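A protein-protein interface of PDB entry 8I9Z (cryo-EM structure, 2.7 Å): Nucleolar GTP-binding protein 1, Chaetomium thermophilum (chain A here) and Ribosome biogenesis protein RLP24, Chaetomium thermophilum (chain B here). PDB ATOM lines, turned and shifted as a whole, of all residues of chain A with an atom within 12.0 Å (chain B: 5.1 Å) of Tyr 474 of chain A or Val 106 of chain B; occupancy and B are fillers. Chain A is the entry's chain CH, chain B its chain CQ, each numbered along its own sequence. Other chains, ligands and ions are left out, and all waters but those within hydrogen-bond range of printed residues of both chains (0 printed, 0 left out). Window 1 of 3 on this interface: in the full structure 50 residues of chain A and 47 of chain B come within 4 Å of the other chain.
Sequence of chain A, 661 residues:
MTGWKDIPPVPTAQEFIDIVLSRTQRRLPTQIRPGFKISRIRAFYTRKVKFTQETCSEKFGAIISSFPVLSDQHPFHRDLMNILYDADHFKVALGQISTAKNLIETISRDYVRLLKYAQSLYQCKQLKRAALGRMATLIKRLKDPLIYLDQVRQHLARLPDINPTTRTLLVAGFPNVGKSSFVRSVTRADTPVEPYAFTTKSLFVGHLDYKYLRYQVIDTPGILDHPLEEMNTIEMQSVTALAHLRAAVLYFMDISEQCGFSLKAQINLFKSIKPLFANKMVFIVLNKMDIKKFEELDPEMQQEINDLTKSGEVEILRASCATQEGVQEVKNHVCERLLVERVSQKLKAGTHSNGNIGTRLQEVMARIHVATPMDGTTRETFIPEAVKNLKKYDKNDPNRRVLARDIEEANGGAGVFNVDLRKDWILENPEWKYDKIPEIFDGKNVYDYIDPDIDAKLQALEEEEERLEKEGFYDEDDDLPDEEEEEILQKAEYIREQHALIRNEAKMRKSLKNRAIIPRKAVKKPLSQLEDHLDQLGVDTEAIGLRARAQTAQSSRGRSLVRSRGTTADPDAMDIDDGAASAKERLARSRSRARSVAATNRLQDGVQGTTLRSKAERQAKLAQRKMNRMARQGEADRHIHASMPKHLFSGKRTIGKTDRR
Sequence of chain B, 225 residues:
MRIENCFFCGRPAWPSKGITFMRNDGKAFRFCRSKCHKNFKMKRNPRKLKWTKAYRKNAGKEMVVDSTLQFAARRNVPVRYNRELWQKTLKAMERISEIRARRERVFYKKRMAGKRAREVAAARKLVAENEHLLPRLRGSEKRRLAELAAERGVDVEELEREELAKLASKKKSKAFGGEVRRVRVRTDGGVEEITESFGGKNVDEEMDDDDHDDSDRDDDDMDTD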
ATOM      1  N   ALA A 460     -28.663  15.964  -8.384  1.00  0.00           N
ATOM      2  CA  ALA A 460     -28.517  14.525  -8.569  1.00  0.00           C
ATOM      3  C   ALA A 460     -27.426  13.963  -7.670  1.00  0.00           C
ATOM      4  O   ALA A 460     -27.526  12.825  -7.196  1.00  0.00           O
ATOM      5  CB  ALA A 460     -28.220  14.212 -10.035  1.00  0.00           C
ATOM      6  N   LEU A 461     -26.371  14.744  -7.433  1.00  0.00           N
ATOM      7  CA  LEU A 461     -25.317  14.316  -6.522  1.00  0.00           C
ATOM      8  C   LEU A 461     -25.813  14.267  -5.083  1.00  0.00           C
ATOM      9  O   LEU A 461     -25.460  13.353  -4.328  1.00  0.00           O
ATOM     10  CB  LEU A 461     -24.116  15.249  -6.642  1.00  0.00           C
ATOM     11  CG  LEU A 461     -22.883  14.868  -5.833  1.00  0.00           C
ATOM     12  CD1 LEU A 461     -22.118  13.753  -6.516  1.00  0.00           C
ATOM     13  CD2 LEU A 461     -22.009  16.077  -5.640  1.00  0.00           C
ATOM     14  N   GLU A 462     -26.627  15.245  -4.681  1.00  0.00           N
ATOM     15  CA  GLU A 462     -27.177  15.236  -3.330  1.00  0.00           C
ATOM     16  C   GLU A 462     -28.203  14.123  -3.154  1.00  0.00           C
ATOM     17  O   GLU A 462     -28.364  13.592  -2.049  1.00  0.00           O
ATOM     18  CB  GLU A 462     -27.794  16.596  -3.000  1.00  0.00           C
ATOM     19  CG  GLU A 462     -26.812  17.772  -2.859  1.00  0.00           C
ATOM     20  CD  GLU A 462     -25.854  17.698  -1.662  1.00  0.00           C
ATOM     21  OE1 GLU A 462     -25.133  18.694  -1.446  1.00  0.00           O
ATOM     22  OE2 GLU A 462     -25.839  16.702  -0.906  1.00  0.00           O
ATOM     23  N   GLU A 463     -28.915  13.768  -4.226  1.00  0.00           N
ATOM     24  CA  GLU A 463     -29.785  12.598  -4.171  1.00  0.00           C
ATOM     25  C   GLU A 463     -28.971  11.321  -4.022  1.00  0.00           C
ATOM     26  O   GLU A 463     -29.404  10.374  -3.355  1.00  0.00           O
ATOM     27  CB  GLU A 463     -30.667  12.531  -5.416  1.00  0.00           C
ATOM     28  CG  GLU A 463     -31.771  13.574  -5.455  1.00  0.00           C
ATOM     29  CD  GLU A 463     -33.021  13.133  -4.716  1.00  0.00           C
ATOM     30  OE1 GLU A 463     -33.061  11.978  -4.242  1.00  0.00           O
ATOM     31  OE2 GLU A 463     -33.965  13.943  -4.608  1.00  0.00           O
ATOM     32  N   GLU A 464     -27.796  11.271  -4.650  1.00  0.00           N
ATOM     33  CA  GLU A 464     -26.883  10.157  -4.424  1.00  0.00           C
ATOM     34  C   GLU A 464     -26.356  10.162  -2.992  1.00  0.00           C
ATOM     35  O   GLU A 464     -26.232   9.102  -2.366  1.00  0.00           O
ATOM     36  CB  GLU A 464     -25.742  10.212  -5.441  1.00  0.00           C
ATOM     37  CG  GLU A 464     -24.462   9.535  -4.995  1.00  0.00           C
ATOM     38  CD  GLU A 464     -23.481   9.337  -6.127  1.00  0.00           C
ATOM     39  OE1 GLU A 464     -23.595   8.318  -6.840  1.00  0.00           O
ATOM     40  OE2 GLU A 464     -22.596  10.199  -6.308  1.00  0.00           O
ATOM     41  N   GLU A 465     -26.061  11.348  -2.453  1.00  0.00           N
ATOM     42  CA  GLU A 465     -25.597  11.460  -1.072  1.00  0.00           C
ATOM     43  C   GLU A 465     -26.669  11.033  -0.078  1.00  0.00           C
ATOM     44  O   GLU A 465     -26.353  10.579   1.027  1.00  0.00           O
ATOM     45  CB  GLU A 465     -25.143  12.890  -0.787  1.00  0.00           C
ATOM     46  CG  GLU A 465     -23.784  13.221  -1.353  1.00  0.00           C
ATOM     47  CD  GLU A 465     -22.737  12.216  -0.924  1.00  0.00           C
ATOM     48  OE1 GLU A 465     -22.462  12.137   0.291  1.00  0.00           O
ATOM     49  OE2 GLU A 465     -22.195  11.500  -1.790  1.00  0.00           O
ATOM     50  N   GLU A 466     -27.939  11.191  -0.442  1.00  0.00           N
ATOM     51  CA  GLU A 466     -29.011  10.701   0.414  1.00  0.00           C
ATOM     52  C   GLU A 466     -29.098   9.177   0.365  1.00  0.00           C
ATOM     53  O   GLU A 466     -29.352   8.530   1.386  1.00  0.00           O
ATOM     54  CB  GLU A 466     -30.333  11.343  -0.007  1.00  0.00           C
ATOM     55  CG  GLU A 466     -31.508  11.070   0.912  1.00  0.00           C
ATOM     56  CD  GLU A 466     -31.367  11.771   2.248  1.00  0.00           C
ATOM     57  OE1 GLU A 466     -30.744  12.852   2.285  1.00  0.00           O
ATOM     58  OE2 GLU A 466     -31.897  11.255   3.256  1.00  0.00           O
ATOM     59  N   ARG A 467     -28.901   8.591  -0.819  1.00  0.00           N
ATOM     60  CA  ARG A 467     -28.929   7.138  -0.945  1.00  0.00           C
ATOM     61  C   ARG A 467     -27.714   6.508  -0.275  1.00  0.00           C
ATOM     62  O   ARG A 467     -27.780   5.379   0.220  1.00  0.00           O
ATOM     63  CB  ARG A 467     -28.993   6.730  -2.418  1.00  0.00           C
ATOM     64  CG  ARG A 467     -30.310   7.017  -3.114  1.00  0.00           C
ATOM     65  CD  ARG A 467     -30.520   6.108  -4.321  1.00  0.00           C
ATOM     66  NE  ARG A 467     -29.329   6.073  -5.160  1.00  0.00           N
ATOM     67  CZ  ARG A 467     -29.139   6.814  -6.245  1.00  0.00           C
ATOM     68  NH1 ARG A 467     -30.076   7.628  -6.702  1.00  0.00           N
ATOM     69  NH2 ARG A 467     -27.976   6.737  -6.887  1.00  0.00           N
ATOM     70  N   LEU A 468     -26.592   7.215  -0.260  1.00  0.00           N
ATOM     71  CA  LEU A 468     -25.393   6.669   0.365  1.00  0.00           C
ATOM     72  C   LEU A 468     -25.483   6.729   1.884  1.00  0.00           C
ATOM     73  O   LEU A 468     -24.843   5.938   2.586  1.00  0.00           O
ATOM     74  CB  LEU A 468     -24.166   7.412  -0.133  1.00  0.00           C
ATOM     75  CG  LEU A 468     -23.694   6.936  -1.504  1.00  0.00           C
ATOM     76  CD1 LEU A 468     -22.768   7.961  -2.103  1.00  0.00           C
ATOM     77  CD2 LEU A 468     -23.030   5.583  -1.424  1.00  0.00           C
ATOM     78  N   GLU A 469     -26.238   7.690   2.413  1.00  0.00           N
ATOM     79  CA  GLU A 469     -26.410   7.763   3.859  1.00  0.00           C
ATOM     80  C   GLU A 469     -27.360   6.679   4.351  1.00  0.00           C
ATOM     81  O   GLU A 469     -27.155   6.111   5.429  1.00  0.00           O
ATOM     82  CB  GLU A 469     -26.919   9.153   4.262  1.00  0.00           C
ATOM     83  CG  GLU A 469     -26.020   9.972   5.222  1.00  0.00           C
ATOM     84  CD  GLU A 469     -25.585   9.272   6.521  1.00  0.00           C
ATOM     85  OE1 GLU A 469     -24.614   9.759   7.135  1.00  0.00           O
ATOM     86  OE2 GLU A 469     -26.229   8.305   6.982  1.00  0.00           O
ATOM     87  N   LYS A 470     -28.396   6.361   3.564  1.00  0.00           N
ATOM     88  CA  LYS A 470     -29.493   5.535   4.070  1.00  0.00           C
ATOM     89  C   LYS A 470     -29.084   4.071   4.227  1.00  0.00           C
ATOM     90  O   LYS A 470     -29.281   3.472   5.290  1.00  0.00           O
ATOM     91  CB  LYS A 470     -30.716   5.671   3.152  1.00  0.00           C
ATOM     92  CG  LYS A 470     -31.557   6.955   3.372  1.00  0.00           C
ATOM     93  CD  LYS A 470     -32.337   6.926   4.693  1.00  0.00           C
ATOM     94  CE  LYS A 470     -33.422   8.010   4.788  1.00  0.00           C
ATOM     95  NZ  LYS A 470     -32.898   9.400   4.637  1.00  0.00           N
ATOM     96  N   GLU A 471     -28.481   3.483   3.199  1.00  0.00           N
ATOM     97  CA  GLU A 471     -27.991   2.113   3.337  1.00  0.00           C
ATOM     98  C   GLU A 471     -26.623   2.036   3.994  1.00  0.00           C
ATOM     99  O   GLU A 471     -26.026   0.954   4.013  1.00  0.00           O
ATOM    100  CB  GLU A 471     -27.955   1.348   1.999  1.00  0.00           C
ATOM    101  CG  GLU A 471     -29.248   1.177   1.142  1.00  0.00           C
ATOM    102  CD  GLU A 471     -30.116   2.397   0.905  1.00  0.00           C
ATOM    103  OE1 GLU A 471     -29.614   3.524   0.941  1.00  0.00           O
ATOM    104  OE2 GLU A 471     -31.331   2.210   0.690  1.00  0.00           O
ATOM    105  N   GLY A 472     -26.089   3.151   4.475  1.00  0.00           N
ATOM    106  CA  GLY A 472     -25.007   3.083   5.431  1.00  0.00           C
ATOM    107  C   GLY A 472     -23.633   2.916   4.827  1.00  0.00           C
ATOM    108  O   GLY A 472     -22.877   2.028   5.232  1.00  0.00           O
ATOM    109  N   PHE A 473     -23.299   3.759   3.851  1.00  0.00           N
ATOM    110  CA  PHE A 473     -21.950   3.822   3.308  1.00  0.00           C
ATOM    111  C   PHE A 473     -20.959   4.477   4.256  1.00  0.00           C
ATOM    112  O   PHE A 473     -19.751   4.374   4.019  1.00  0.00           O
ATOM    113  CB  PHE A 473     -21.985   4.584   1.991  1.00  0.00           C
ATOM    114  CG  PHE A 473     -20.870   4.256   1.069  1.00  0.00           C
ATOM    115  CD1 PHE A 473     -20.675   2.965   0.620  1.00  0.00           C
ATOM    116  CD2 PHE A 473     -20.042   5.263   0.604  1.00  0.00           C
ATOM    117  CE1 PHE A 473     -19.642   2.679  -0.254  1.00  0.00           C
ATOM    118  CE2 PHE A 473     -19.015   4.987  -0.273  1.00  0.00           C
ATOM    119  CZ  PHE A 473     -18.813   3.698  -0.702  1.00  0.00           C
ATOM    120  N   TYR A 474     -21.426   5.126   5.329  1.00  0.00           N
ATOM    121  CA  TYR A 474     -20.554   5.890   6.211  1.00  0.00           C
ATOM    122  C   TYR A 474     -20.689   5.501   7.685  1.00  0.00           C
ATOM    123  O   TYR A 474     -20.291   6.275   8.563  1.00  0.00           O
ATOM    124  CB  TYR A 474     -20.832   7.376   6.024  1.00  0.00           C
ATOM    125  CG  TYR A 474     -20.783   7.834   4.580  1.00  0.00           C
ATOM    126  CD1 TYR A 474     -19.574   8.021   3.922  1.00  0.00           C
ATOM    127  CD2 TYR A 474     -21.952   8.107   3.884  1.00  0.00           C
ATOM    128  CE1 TYR A 474     -19.540   8.467   2.616  1.00  0.00           C
ATOM    129  CE2 TYR A 474     -21.924   8.518   2.570  1.00  0.00           C
ATOM    130  CZ  TYR A 474     -20.717   8.702   1.950  1.00  0.00           C
ATOM    131  OH  TYR A 474     -20.673   9.151   0.658  1.00  0.00           O
ATOM    132  N   ASP A 475     -21.224   4.318   7.983  1.00  0.00           N
ATOM    133  CA  ASP A 475     -21.360   3.878   9.364  1.00  0.00           C
ATOM    134  C   ASP A 475     -20.107   3.138   9.816  1.00  0.00           C
ATOM    135  O   ASP A 475     -19.438   2.464   9.028  1.00  0.00           O
ATOM    136  CB  ASP A 475     -22.592   2.987   9.540  1.00  0.00           C
ATOM    137  CG  ASP A 475     -23.879   3.790   9.625  1.00  0.00           C
ATOM    138  OD1 ASP A 475     -23.986   4.650  10.528  1.00  0.00           O
ATOM    139  OD2 ASP A 475     -24.775   3.574   8.781  1.00  0.00           O
ATOM    140  N   GLU A 476     -19.793   3.278  11.100  1.00  0.00           N
ATOM    141  CA  GLU A 476     -18.641   2.624  11.703  1.00  0.00           C
ATOM    142  C   GLU A 476     -19.083   1.352  12.410  1.00  0.00           C
ATOM    143  O   GLU A 476     -20.003   1.382  13.234  1.00  0.00           O
ATOM    144  CB  GLU A 476     -17.934   3.556  12.690  1.00  0.00           C
ATOM    145  CG  GLU A 476     -16.707   2.938  13.345  1.00  0.00           C
ATOM    146  CD  GLU A 476     -16.028   3.877  14.323  1.00  0.00           C
ATOM    147  OE1 GLU A 476     -16.556   4.989  14.549  1.00  0.00           O
ATOM    148  OE2 GLU A 476     -14.968   3.502  14.866  1.00  0.00           O
ATOM    149  N   ASP A 477     -18.422   0.244  12.092  1.00  0.00           N
ATOM    150  CA  ASP A 477     -18.755  -1.047  12.685  1.00  0.00           C
ATOM    151  C   ASP A 477     -17.571  -1.624  13.457  1.00  0.00           C
ATOM    152  O   ASP A 477     -16.465  -1.734  12.927  1.00  0.00           O
ATOM    153  CB  ASP A 477     -19.206  -2.029  11.602  1.00  0.00           C
ATOM    154  CG  ASP A 477     -20.528  -1.635  10.974  1.00  0.00           C
ATOM    155  OD1 ASP A 477     -21.531  -1.536  11.711  1.00  0.00           O
ATOM    156  OD2 ASP A 477     -20.560  -1.420   9.745  1.00  0.00           O
ATOM    157  N   ARG B 102     -14.923  13.035   2.039  1.00  0.00           N
ATOM    158  CA  ARG B 102     -15.651  12.060   2.826  1.00  0.00           C
ATOM    159  C   ARG B 102     -15.806  10.753   2.056  1.00  0.00           C
ATOM    160  O   ARG B 102     -16.208   9.730   2.621  1.00  0.00           O
ATOM    161  CB  ARG B 102     -16.983  12.674   3.238  1.00  0.00           C
ATOM    162  CG  ARG B 102     -17.555  12.133   4.518  1.00  0.00           C
ATOM    163  CD  ARG B 102     -18.835  12.901   4.850  1.00  0.00           C
ATOM    164  NE  ARG B 102     -19.889  12.701   3.866  1.00  0.00           N
ATOM    165  CZ  ARG B 102     -20.807  11.751   3.938  1.00  0.00           C
ATOM    166  NH1 ARG B 102     -20.844  10.908   4.947  1.00  0.00           N
ATOM    167  NH2 ARG B 102     -21.725  11.658   2.983  1.00  0.00           N
ATOM    168  N   ARG B 103     -15.501  10.774   0.757  1.00  0.00           N
ATOM    169  CA  ARG B 103     -15.436   9.535  -0.008  1.00  0.00           C
ATOM    170  C   ARG B 103     -14.000   9.058  -0.167  1.00  0.00           C
ATOM    171  O   ARG B 103     -13.762   7.861  -0.343  1.00  0.00           O
ATOM    172  CB  ARG B 103     -16.095   9.718  -1.371  1.00  0.00           C
ATOM    173  CG  ARG B 103     -17.595   9.925  -1.312  1.00  0.00           C
ATOM    174  CD  ARG B 103     -18.182   9.807  -2.691  1.00  0.00           C
ATOM    175  NE  ARG B 103     -19.567  10.250  -2.771  1.00  0.00           N
ATOM    176  CZ  ARG B 103     -20.248  10.305  -3.906  1.00  0.00           C
ATOM    177  NH1 ARG B 103     -19.698   9.960  -5.056  1.00  0.00           N
ATOM    178  NH2 ARG B 103     -21.505  10.739  -3.889  1.00  0.00           N
ATOM    179  N   GLU B 104     -13.030   9.980  -0.129  1.00  0.00           N
ATOM    180  CA  GLU B 104     -11.626   9.581  -0.056  1.00  0.00           C
ATOM    181  C   GLU B 104     -11.342   8.799   1.218  1.00  0.00           C
ATOM    182  O   GLU B 104     -10.577   7.829   1.205  1.00  0.00           O
ATOM    183  CB  GLU B 104     -10.710  10.807  -0.101  1.00  0.00           C
ATOM    184  CG  GLU B 104     -10.440  11.460  -1.458  1.00  0.00           C
ATOM    185  CD  GLU B 104     -10.154  10.463  -2.560  1.00  0.00           C
ATOM    186  OE1 GLU B 104      -9.210   9.656  -2.408  1.00  0.00           O
ATOM    187  OE2 GLU B 104     -10.837  10.519  -3.600  1.00  0.00           O
ATOM    188  N   ARG B 105     -11.945   9.219   2.331  1.00  0.00           N
ATOM    189  CA  ARG B 105     -11.672   8.605   3.626  1.00  0.00           C
ATOM    190  C   ARG B 105     -12.258   7.200   3.704  1.00  0.00           C
ATOM    191  O   ARG B 105     -11.664   6.299   4.308  1.00  0.00           O
ATOM    192  CB  ARG B 105     -12.225   9.512   4.725  1.00  0.00           C
ATOM    193  CG  ARG B 105     -12.485   8.868   6.062  1.00  0.00           C
ATOM    194  CD  ARG B 105     -11.202   8.777   6.856  1.00  0.00           C
ATOM    195  NE  ARG B 105     -11.006   9.951   7.697  1.00  0.00           N
ATOM    196  CZ  ARG B 105     -10.349   9.947   8.848  1.00  0.00           C
ATOM    197  NH1 ARG B 105      -9.807   8.841   9.331  1.00  0.00           N
ATOM    198  NH2 ARG B 105     -10.227  11.082   9.529  1.00  0.00           N
ATOM    199  N   VAL B 106     -13.419   6.992   3.079  1.00  0.00           N
ATOM    200  CA  VAL B 106     -14.037   5.670   3.045  1.00  0.00           C
ATOM    201  C   VAL B 106     -13.221   4.723   2.174  1.00  0.00           C
ATOM    202  O   VAL B 106     -13.064   3.537   2.493  1.00  0.00           O
ATOM    203  CB  VAL B 106     -15.499   5.794   2.571  1.00  0.00           C
ATOM    204  CG1 VAL B 106     -16.098   4.440   2.207  1.00  0.00           C
ATOM    205  CG2 VAL B 106     -16.329   6.485   3.632  1.00  0.00           C
ATOM    206  N   PHE B 107     -12.666   5.239   1.075  1.00  0.00           N
ATOM    207  CA  PHE B 107     -11.832   4.430   0.192  1.00  0.00           C
ATOM    208  C   PHE B 107     -10.565   3.962   0.898  1.00  0.00           C
ATOM    209  O   PHE B 107     -10.092   2.843   0.671  1.00  0.00           O
ATOM    210  CB  PHE B 107     -11.473   5.231  -1.058  1.00  0.00           C
ATOM    211  CG  PHE B 107     -10.989   4.390  -2.198  1.00  0.00           C
ATOM    212  CD1 PHE B 107     -11.791   3.399  -2.736  1.00  0.00           C
ATOM    213  CD2 PHE B 107      -9.723   4.575  -2.717  1.00  0.00           C
ATOM    214  CE1 PHE B 107     -11.342   2.620  -3.784  1.00  0.00           C
ATOM    215  CE2 PHE B 107      -9.268   3.796  -3.760  1.00  0.00           C
ATOM    216  CZ  PHE B 107     -10.075   2.820  -4.293  1.00  0.00           C
ATOM    217  N   TYR B 108      -9.995   4.812   1.752  1.00  0.00           N
ATOM    218  CA  TYR B 108      -8.771   4.447   2.459  1.00  0.00           C
ATOM    219  C   TYR B 108      -9.047   3.435   3.564  1.00  0.00           C
ATOM    220  O   TYR B 108      -8.228   2.545   3.822  1.00  0.00           O
ATOM    221  CB  TYR B 108      -8.102   5.696   3.026  1.00  0.00           C
ATOM    222  CG  TYR B 108      -6.662   5.482   3.417  1.00  0.00           C
ATOM    223  CD1 TYR B 108      -5.675   5.351   2.455  1.00  0.00           C
ATOM    224  CD2 TYR B 108      -6.291   5.411   4.749  1.00  0.00           C
ATOM    225  CE1 TYR B 108      -4.363   5.155   2.808  1.00  0.00           C
ATOM    226  CE2 TYR B 108      -4.975   5.215   5.111  1.00  0.00           C
ATOM    227  CZ  TYR B 108      -4.018   5.089   4.137  1.00  0.00           C
ATOM    228  OH  TYR B 108      -2.706   4.893   4.492  1.00  0.00           O
ATOM    229  N   LYS B 109     -10.191   3.566   4.240  1.00  0.00           N
ATOM    230  CA  LYS B 109     -10.563   2.604   5.274  1.00  0.00           C
ATOM    231  C   LYS B 109     -10.840   1.228   4.682  1.00  0.00           C
ATOM    232  O   LYS B 109     -10.633   0.206   5.346  1.00  0.00           O
ATOM    233  CB  LYS B 109     -11.784   3.106   6.043  1.00  0.00           C
ATOM    234  CG  LYS B 109     -11.486   3.857   7.325  1.00  0.00           C
ATOM    235  CD  LYS B 109     -12.728   4.587   7.802  1.00  0.00           C
ATOM    236  CE  LYS B 109     -12.545   5.227   9.170  1.00  0.00           C
ATOM    237  NZ  LYS B 109     -11.324   4.756   9.871  1.00  0.00           N
ATOM    238  N   LYS B 110     -11.320   1.181   3.439  1.00  0.00           N
ATOM    239  CA  LYS B 110     -11.605  -0.097   2.800  1.00  0.00           C
ATOM    240  C   LYS B 110     -10.326  -0.835   2.425  1.00  0.00           C
ATOM    241  O   LYS B 110     -10.273  -2.068   2.511  1.00  0.00           O
ATOM    242  CB  LYS B 110     -12.490   0.129   1.573  1.00  0.00           C
ATOM    243  CG  LYS B 110     -12.853  -1.131   0.797  1.00  0.00           C
ATOM    244  CD  LYS B 110     -14.000  -0.919  -0.202  1.00  0.00           C
ATOM    245  CE  LYS B 110     -15.172  -0.062   0.305  1.00  0.00           C
ATOM    246  NZ  LYS B 110     -15.660  -0.344   1.694  1.00  0.00           N
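Leu 461 of chain A touches none of the printed residues of chain B. Of the printed residues of chain B, Glu 464 of chain A touches Arg 103. Of the printed residues of chain B, Glu 465 of chain A touches Arg 102 (2.8 Å) and Arg 103 (2.3 Å). Of the printed residues of chain B, Leu 468 of chain A touches Arg 103. Of the printed residues of chain B, Phe 473 of chain A touches Val 106 (3.9 Å). Tyr 474 of chain A touches just these residues of chain B: Arg 102 (3.1 Å), Arg 103 (3.7 Å) and Val 106 (3.6 Å). Glu 476 of chain A touches none of the printed residues of chain B. Of chain A, only Glu 465 and Tyr 474 come within 4 Å of Arg 102 of chain B. Of chain A, only Glu 464, Glu 465, Leu 468 and Tyr 474 come within 4 Å of Arg 103 of chain B. Of chain A, only Phe 473 and Tyr 474 come within 4 Å of Val 106 of chain B. No residue of chain A comes within 4 Å of Phe 107 of chain B. No residue of chain A comes within 4 Å of Lys 110 of chain B. The nearest residue of chain A that does not touch Val 106 of chain B is Asp 475 of chain A (6.9 Å). The nearest printed residue of chain B that does not touch Phe 473 of chain A is Arg 103 of chain B (5.2 Å).
OE1 of Glu 465 of chain A sits close to OH of Tyr 474 of chain A (3.5 Å). The backbone carbonyl oxygen (O) of Leu 468 of chain A lies within hydrogen-bond range of the backbone NH (N) of Phe 473 of chain A, at 3.0 Å.
The guanidinium group of Arg 103 of chain B is in salt-bridge range of the side-chain carboxylate of Glu 465 of chain A (3.1 Å). OE2 of Glu 464 of chain A lies within salt-bridge range of NH2 of Arg 103 of chain B (2.7 Å). The guanidinium group of Arg 102 of chain B is in salt-bridge range of the side-chain carboxylate of Glu 465 of chain A (2.8 Å).
Of the 9 printed residues of chain B, 3 touch a printed residue of chain A. Hydrophobic or aromatic side chains of chain B within 4 Å of the printed part of chain A: Val 106. Of the 18 printed residues of chain A, 5 touch a printed residue of chain B. Among the printed residues, 8 pairs touch across the chains. Among the printed residues, Asp or Glu carboxylates within 4 Å of a Lys or Arg side-chain nitrogen of the other chain: Glu 464 of chain A with Arg 103 of chain B, Glu 465 of chain A with Arg 102 of chain B and Glu 465 of chain A with Arg 103 of chain B.
Leu 468 of chain A touches Arg 103 of chain B (CD1 to NH2, 3.5 Å). Phe 473 of chain A touches Val 106 of chain B (CE2 to CG1, 3.9 Å). Arg 102 of chain B touches Tyr 474 of chain A. CG of Arg 103 of chain B touches OH of Tyr 474 of chain A, 3.7 Å away. Tyr 474 of chain A touches Val 106 of chain B (CD1 to CG2, 3.6 Å).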
